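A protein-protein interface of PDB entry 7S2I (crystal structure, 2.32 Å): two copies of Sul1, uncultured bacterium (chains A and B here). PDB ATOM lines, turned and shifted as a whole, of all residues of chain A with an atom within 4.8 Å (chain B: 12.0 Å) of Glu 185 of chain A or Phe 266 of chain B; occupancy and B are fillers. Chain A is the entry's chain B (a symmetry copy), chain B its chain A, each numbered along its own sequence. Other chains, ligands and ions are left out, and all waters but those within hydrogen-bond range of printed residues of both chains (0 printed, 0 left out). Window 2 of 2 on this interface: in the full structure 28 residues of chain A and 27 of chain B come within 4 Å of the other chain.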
ATOM      1  N   PRO A 142      19.604  -1.963  14.728  1.00  0.00           N
ATOM      2  CA  PRO A 142      19.697  -3.407  15.021  1.00  0.00           C
ATOM      3  C   PRO A 142      19.187  -4.293  13.901  1.00  0.00           C
ATOM      4  O   PRO A 142      19.782  -5.344  13.624  1.00  0.00           O
ATOM      5  CB  PRO A 142      18.842  -3.556  16.289  1.00  0.00           C
ATOM      6  CG  PRO A 142      18.854  -2.209  16.915  1.00  0.00           C
ATOM      7  CD  PRO A 142      18.897  -1.226  15.789  1.00  0.00           C
ATOM      8  N   ALA A 183      23.747   4.651  19.833  1.00  0.00           N
ATOM      9  CA  ALA A 183      22.698   4.112  20.677  1.00  0.00           C
ATOM     10  C   ALA A 183      23.072   2.718  21.163  1.00  0.00           C
ATOM     11  O   ALA A 183      23.674   1.940  20.415  1.00  0.00           O
ATOM     12  CB  ALA A 183      21.371   4.052  19.915  1.00  0.00           C
ATOM     13  N   PRO A 184      22.728   2.378  22.407  1.00  0.00           N
ATOM     14  CA  PRO A 184      23.108   1.057  22.937  1.00  0.00           C
ATOM     15  C   PRO A 184      22.419  -0.106  22.239  1.00  0.00           C
ATOM     16  O   PRO A 184      22.963  -1.218  22.253  1.00  0.00           O
ATOM     17  CB  PRO A 184      22.678   1.128  24.413  1.00  0.00           C
ATOM     18  CG  PRO A 184      22.235   2.546  24.658  1.00  0.00           C
ATOM     19  CD  PRO A 184      21.859   3.117  23.335  1.00  0.00           C
ATOM     20  N   GLU A 185      21.247   0.116  21.632  1.00  0.00           N
ATOM     21  CA  GLU A 185      20.403  -0.996  21.194  1.00  0.00           C
ATOM     22  C   GLU A 185      21.114  -1.890  20.188  1.00  0.00           C
ATOM     23  O   GLU A 185      20.907  -3.108  20.181  1.00  0.00           O
ATOM     24  CB  GLU A 185      19.102  -0.463  20.593  1.00  0.00           C
ATOM     25  CG  GLU A 185      18.113   0.038  21.620  1.00  0.00           C
ATOM     26  CD  GLU A 185      18.484   1.408  22.147  1.00  0.00           C
ATOM     27  OE1 GLU A 185      19.299   2.093  21.495  1.00  0.00           O
ATOM     28  OE2 GLU A 185      17.970   1.793  23.219  1.00  0.00           O
ATOM     29  N   THR A 186      21.942  -1.304  19.322  1.00  0.00           N
ATOM     30  CA  THR A 186      22.598  -2.092  18.282  1.00  0.00           C
ATOM     31  C   THR A 186      23.677  -3.000  18.863  1.00  0.00           C
ATOM     32  O   THR A 186      23.770  -4.177  18.491  1.00  0.00           O
ATOM     33  CB  THR A 186      23.173  -1.170  17.208  1.00  0.00           C
ATOM     34  OG1 THR A 186      22.160  -0.244  16.787  1.00  0.00           O
ATOM     35  CG2 THR A 186      23.677  -1.975  16.020  1.00  0.00           C
ATOM     36  N   SER A 187      24.506  -2.476  19.772  1.00  0.00           N
ATOM     37  CA  SER A 187      25.445  -3.345  20.480  1.00  0.00           C
ATOM     38  C   SER A 187      24.716  -4.436  21.253  1.00  0.00           C
ATOM     39  O   SER A 187      25.142  -5.597  21.249  1.00  0.00           O
ATOM     40  CB  SER A 187      26.332  -2.534  21.427  1.00  0.00           C
ATOM     41  OG  SER A 187      27.064  -1.536  20.739  1.00  0.00           O
ATOM     42  N   LEU A 188      23.614  -4.089  21.921  1.00  0.00           N
ATOM     43  CA  LEU A 188      22.882  -5.096  22.680  1.00  0.00           C
ATOM     44  C   LEU A 188      22.324  -6.171  21.759  1.00  0.00           C
ATOM     45  O   LEU A 188      22.408  -7.365  22.068  1.00  0.00           O
ATOM     46  CB  LEU A 188      21.763  -4.439  23.488  1.00  0.00           C
ATOM     47  CG  LEU A 188      22.271  -3.541  24.620  1.00  0.00           C
ATOM     48  CD1 LEU A 188      21.131  -2.745  25.229  1.00  0.00           C
ATOM     49  CD2 LEU A 188      22.992  -4.356  25.693  1.00  0.00           C
ATOM     50  N   HIS A 189      21.767  -5.769  20.616  1.00  0.00           N
ATOM     51  CA  HIS A 189      21.223  -6.744  19.679  1.00  0.00           C
ATOM     52  C   HIS A 189      22.321  -7.639  19.114  1.00  0.00           C
ATOM     53  O   HIS A 189      22.148  -8.860  19.007  1.00  0.00           O
ATOM     54  CB  HIS A 189      20.499  -6.029  18.540  1.00  0.00           C
ATOM     55  CG  HIS A 189      19.966  -6.955  17.492  1.00  0.00           C
ATOM     56  ND1 HIS A 189      19.222  -8.075  17.797  1.00  0.00           N
ATOM     57  CD2 HIS A 189      20.111  -6.955  16.146  1.00  0.00           C
ATOM     58  CE1 HIS A 189      18.901  -8.704  16.680  1.00  0.00           C
ATOM     59  NE2 HIS A 189      19.431  -8.047  15.665  1.00  0.00           N
ATOM     60  N   SER A 192      23.618  -9.887  21.966  1.00  0.00           N
ATOM     61  CA  SER A 192      22.605 -10.855  22.360  1.00  0.00           C
ATOM     62  C   SER A 192      22.463 -11.970  21.336  1.00  0.00           C
ATOM     63  O   SER A 192      22.101 -13.096  21.693  1.00  0.00           O
ATOM     64  CB  SER A 192      21.266 -10.151  22.577  1.00  0.00           C
ATOM     65  OG  SER A 192      20.227 -11.079  22.792  1.00  0.00           O
ATOM     66  N   ASN A 193      22.763 -11.701  20.072  1.00  0.00           N
ATOM     67  CA  ASN A 193      22.539 -12.701  19.041  1.00  0.00           C
ATOM     68  C   ASN A 193      23.856 -13.035  18.349  1.00  0.00           C
ATOM     69  O   ASN A 193      23.913 -13.265  17.135  1.00  0.00           O
ATOM     70  CB  ASN A 193      21.481 -12.231  18.045  1.00  0.00           C
ATOM     71  CG  ASN A 193      20.143 -11.950  18.716  1.00  0.00           C
ATOM     72  OD1 ASN A 193      19.708 -10.801  18.776  1.00  0.00           O
ATOM     73  ND2 ASN A 193      19.544 -12.975  19.326  1.00  0.00           N
ATOM     74  N   ILE B 257      23.297  -7.636  37.219  1.00  0.00           N
ATOM     75  CA  ILE B 257      21.930  -8.124  37.027  1.00  0.00           C
ATOM     76  C   ILE B 257      21.195  -7.236  36.029  1.00  0.00           C
ATOM     77  O   ILE B 257      20.555  -7.724  35.091  1.00  0.00           O
ATOM     78  CB  ILE B 257      21.178  -8.186  38.371  1.00  0.00           C
ATOM     79  CG1 ILE B 257      21.794  -9.233  39.299  1.00  0.00           C
ATOM     80  CG2 ILE B 257      19.678  -8.505  38.156  1.00  0.00           C
ATOM     81  CD1 ILE B 257      21.166  -9.249  40.720  1.00  0.00           C
ATOM     82  N   THR B 258      21.284  -5.915  36.221  1.00  0.00           N
ATOM     83  CA  THR B 258      20.623  -4.977  35.319  1.00  0.00           C
ATOM     84  C   THR B 258      21.078  -5.182  33.878  1.00  0.00           C
ATOM     85  O   THR B 258      20.260  -5.148  32.953  1.00  0.00           O
ATOM     86  CB  THR B 258      20.890  -3.541  35.776  1.00  0.00           C
ATOM     87  OG1 THR B 258      20.247  -3.324  37.038  1.00  0.00           O
ATOM     88  CG2 THR B 258      20.345  -2.527  34.765  1.00  0.00           C
ATOM     89  N   PHE B 259      22.373  -5.412  33.666  1.00  0.00           N
ATOM     90  CA  PHE B 259      22.833  -5.672  32.307  1.00  0.00           C
ATOM     91  C   PHE B 259      22.257  -6.974  31.763  1.00  0.00           C
ATOM     92  O   PHE B 259      21.841  -7.037  30.599  1.00  0.00           O
ATOM     93  CB  PHE B 259      24.356  -5.734  32.239  1.00  0.00           C
ATOM     94  CG  PHE B 259      24.845  -6.234  30.924  1.00  0.00           C
ATOM     95  CD1 PHE B 259      24.946  -5.368  29.844  1.00  0.00           C
ATOM     96  CD2 PHE B 259      25.125  -7.580  30.732  1.00  0.00           C
ATOM     97  CE1 PHE B 259      25.358  -5.827  28.606  1.00  0.00           C
ATOM     98  CE2 PHE B 259      25.529  -8.049  29.489  1.00  0.00           C
ATOM     99  CZ  PHE B 259      25.653  -7.171  28.432  1.00  0.00           C
ATOM    100  N   SER B 260      22.256  -8.032  32.581  1.00  0.00           N
ATOM    101  CA  SER B 260      21.784  -9.338  32.120  1.00  0.00           C
ATOM    102  C   SER B 260      20.307  -9.295  31.759  1.00  0.00           C
ATOM    103  O   SER B 260      19.894  -9.842  30.728  1.00  0.00           O
ATOM    104  CB  SER B 260      22.027 -10.396  33.198  1.00  0.00           C
ATOM    105  OG  SER B 260      23.362 -10.869  33.166  1.00  0.00           O
ATOM    106  N   GLU B 261      19.492  -8.657  32.600  1.00  0.00           N
ATOM    107  CA  GLU B 261      18.064  -8.581  32.321  1.00  0.00           C
ATOM    108  C   GLU B 261      17.785  -7.728  31.091  1.00  0.00           C
ATOM    109  O   GLU B 261      16.918  -8.070  30.278  1.00  0.00           O
ATOM    110  CB  GLU B 261      17.323  -8.053  33.551  1.00  0.00           C
ATOM    111  CG  GLU B 261      17.544  -8.909  34.810  1.00  0.00           C
ATOM    112  CD  GLU B 261      16.797  -8.389  36.041  1.00  0.00           C
ATOM    113  OE1 GLU B 261      16.708  -7.147  36.199  1.00  0.00           O
ATOM    114  OE2 GLU B 261      16.320  -9.219  36.858  1.00  0.00           O
ATOM    115  N   THR B 262      18.519  -6.624  30.924  1.00  0.00           N
ATOM    116  CA  THR B 262      18.340  -5.809  29.726  1.00  0.00           C
ATOM    117  C   THR B 262      18.753  -6.581  28.480  1.00  0.00           C
ATOM    118  O   THR B 262      18.101  -6.481  27.435  1.00  0.00           O
ATOM    119  CB  THR B 262      19.142  -4.507  29.837  1.00  0.00           C
ATOM    120  OG1 THR B 262      18.717  -3.773  30.989  1.00  0.00           O
ATOM    121  CG2 THR B 262      18.932  -3.636  28.599  1.00  0.00           C
ATOM    122  N   LEU B 263      19.828  -7.368  28.573  1.00  0.00           N
ATOM    123  CA  LEU B 263      20.323  -8.082  27.402  1.00  0.00           C
ATOM    124  C   LEU B 263      19.357  -9.172  26.958  1.00  0.00           C
ATOM    125  O   LEU B 263      19.195  -9.404  25.750  1.00  0.00           O
ATOM    126  CB  LEU B 263      21.695  -8.675  27.706  1.00  0.00           C
ATOM    127  CG  LEU B 263      22.419  -9.373  26.564  1.00  0.00           C
ATOM    128  CD1 LEU B 263      22.756  -8.364  25.488  1.00  0.00           C
ATOM    129  CD2 LEU B 263      23.685  -9.999  27.101  1.00  0.00           C
ATOM    130  N   ALA B 264      18.702  -9.841  27.913  1.00  0.00           N
ATOM    131  CA  ALA B 264      17.744 -10.887  27.576  1.00  0.00           C
ATOM    132  C   ALA B 264      16.579 -10.359  26.754  1.00  0.00           C
ATOM    133  O   ALA B 264      15.963 -11.129  26.011  1.00  0.00           O
ATOM    134  CB  ALA B 264      17.217 -11.559  28.848  1.00  0.00           C
ATOM    135  N   LYS B 265      16.264  -9.066  26.860  1.00  0.00           N
ATOM    136  CA  LYS B 265      15.150  -8.525  26.092  1.00  0.00           C
ATOM    137  C   LYS B 265      15.454  -8.426  24.604  1.00  0.00           C
ATOM    138  O   LYS B 265      14.525  -8.249  23.811  1.00  0.00           O
ATOM    139  CB  LYS B 265      14.751  -7.150  26.630  1.00  0.00           C
ATOM    140  CG  LYS B 265      14.441  -7.128  28.123  1.00  0.00           C
ATOM    141  CD  LYS B 265      14.035  -5.731  28.568  1.00  0.00           C
ATOM    142  CE  LYS B 265      13.277  -5.756  29.880  1.00  0.00           C
ATOM    143  NZ  LYS B 265      13.384  -4.444  30.579  1.00  0.00           N
ATOM    144  N   PHE B 266      16.720  -8.537  24.205  1.00  0.00           N
ATOM    145  CA  PHE B 266      17.086  -8.453  22.796  1.00  0.00           C
ATOM    146  C   PHE B 266      17.216  -9.814  22.128  1.00  0.00           C
ATOM    147  O   PHE B 266      17.441  -9.874  20.913  1.00  0.00           O
ATOM    148  CB  PHE B 266      18.391  -7.661  22.635  1.00  0.00           C
ATOM    149  CG  PHE B 266      18.223  -6.199  22.880  1.00  0.00           C
ATOM    150  CD1 PHE B 266      18.180  -5.703  24.172  1.00  0.00           C
ATOM    151  CD2 PHE B 266      18.054  -5.322  21.820  1.00  0.00           C
ATOM    152  CE1 PHE B 266      17.997  -4.360  24.407  1.00  0.00           C
ATOM    153  CE2 PHE B 266      17.874  -3.974  22.046  1.00  0.00           C
ATOM    154  CZ  PHE B 266      17.844  -3.493  23.345  1.00  0.00           C
ATOM    155  N   ARG B 267      17.069 -10.899  22.883  1.00  0.00           N
ATOM    156  CA  ARG B 267      17.159 -12.235  22.308  1.00  0.00           C
ATOM    157  C   ARG B 267      15.997 -12.479  21.352  1.00  0.00           C
ATOM    158  O   ARG B 267      14.842 -12.178  21.669  1.00  0.00           O
ATOM    159  CB  ARG B 267      17.173 -13.281  23.422  1.00  0.00           C
ATOM    160  CG  ARG B 267      17.739 -14.630  23.007  1.00  0.00           C
ATOM    161  CD  ARG B 267      19.212 -14.522  22.637  1.00  0.00           C
ATOM    162  NE  ARG B 267      19.830 -15.824  22.406  1.00  0.00           N
ATOM    163  CZ  ARG B 267      20.583 -16.470  23.288  1.00  0.00           C
ATOM    164  NH1 ARG B 267      20.848 -15.958  24.480  1.00  0.00           N
ATOM    165  NH2 ARG B 267      21.089 -17.657  22.964  1.00  0.00           N
ATOM    166  N   SER B 268      16.306 -13.021  20.178  1.00  0.00           N
ATOM    167  CA  SER B 268      15.290 -13.292  19.167  1.00  0.00           C
ATOM    168  C   SER B 268      14.694 -14.688  19.334  1.00  0.00           C
ATOM    169  O   SER B 268      13.625 -14.987  18.798  1.00  0.00           O
ATOM    170  CB  SER B 268      15.882 -13.137  17.767  1.00  0.00           C
ATOM    171  OG  SER B 268      15.981 -11.770  17.406  1.00  0.00           O
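A ring nitrogen (NE2) of His 189 of chain A lies close to the backbone carbonyl oxygen (O) of Pro 142 of chain A, 3.4 Å away. A ring nitrogen (ND1) of His 189 of chain A is in hydrogen-bond range of the side-chain amide oxygen (OD1) of Asn 193 of chain A.
Among the printed residues, merely in contact across the chains: Ser 192 of chain A with Phe 266 of chain B (3.3 Å), Ser 192 of chain A with Leu 263 of chain B (3.6 Å), Leu 188 of chain A with Leu 263 of chain B (3.6 Å), Leu 188 of chain A with Phe 266 of chain B (3.6 Å), Glu 185 of chain A with Phe 266 of chain B (3.7 Å), Asn 193 of chain A with Arg 267 of chain B (3.7 Å) and His 189 of chain A with Phe 266 of chain B (3.9 Å).
The backbone carbonyl oxygen of Phe 266 of chain B lies close to the side-chain amide oxygen of Asn 193 of chain A (3.3 Å). The side-chain hydroxyl (OG) of Ser 192 of chain A lies within hydrogen-bond range of the backbone NH (N) of Arg 267 of chain B (3.2 Å). N of Ser 268 of chain B sits close to ND2 of Asn 193 of chain A.
No residue of chain B comes within 4 Å of Pro 142 of chain A. No residue of chain B comes within 4 Å of Ala 183 of chain A. No residue of chain B comes within 4 Å of Pro 184 of chain A. Glu 185 of chain A touches just one residue of chain B: Phe 266. Ser 187 of chain A touches none of the printed residues of chain B. Leu 188 of chain A touches just these residues of chain B: Leu 263 (3.6 Å) and Phe 266 (3.6 Å). His 189 of chain A touches just one residue of chain B: Phe 266. Printed residues of chain B within 4 Å of Asn 193 of chain A: Phe 266 (3.3 Å), Arg 267 (3.7 Å) and Ser 268 (3.3 Å). Of the printed residues of chain A, Leu 263 of chain B touches Leu 188 (3.6 Å) and Ser 192 (3.6 Å). Lys 265 of chain B touches none of the printed residues of chain A. Printed residues of chain A within 4 Å of Arg 267 of chain B: Ser 192 (3.2 Å) and Asn 193 (3.7 Å). Of the printed residues of chain A, Ser 268 of chain B touches Asn 193 (3.3 Å). The nearest printed residue of chain B that does not touch Glu 185 of chain A is Leu 263 of chain B (7.7 Å).
Printed residues of chain B that touch a printed residue of chain A: Leu 263, Phe 266, Arg 267 and Ser 268. Hydrophobic or aromatic side chains of chain B that line the printed part of chain A: Leu 263 and Phe 266. Printed residues of chain A that touch a printed residue of chain B: Glu 185, Leu 188, His 189, Ser 192 and Asn 193. Hydrophobic or aromatic side chains of chain A within 4 Å of the printed part of chain B: Leu 188. Among the printed residues, no Asp or Glu carboxylate lies within 4 Å of a Lys or Arg side-chain nitrogen of the other chain.
No position is printed for both chains.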
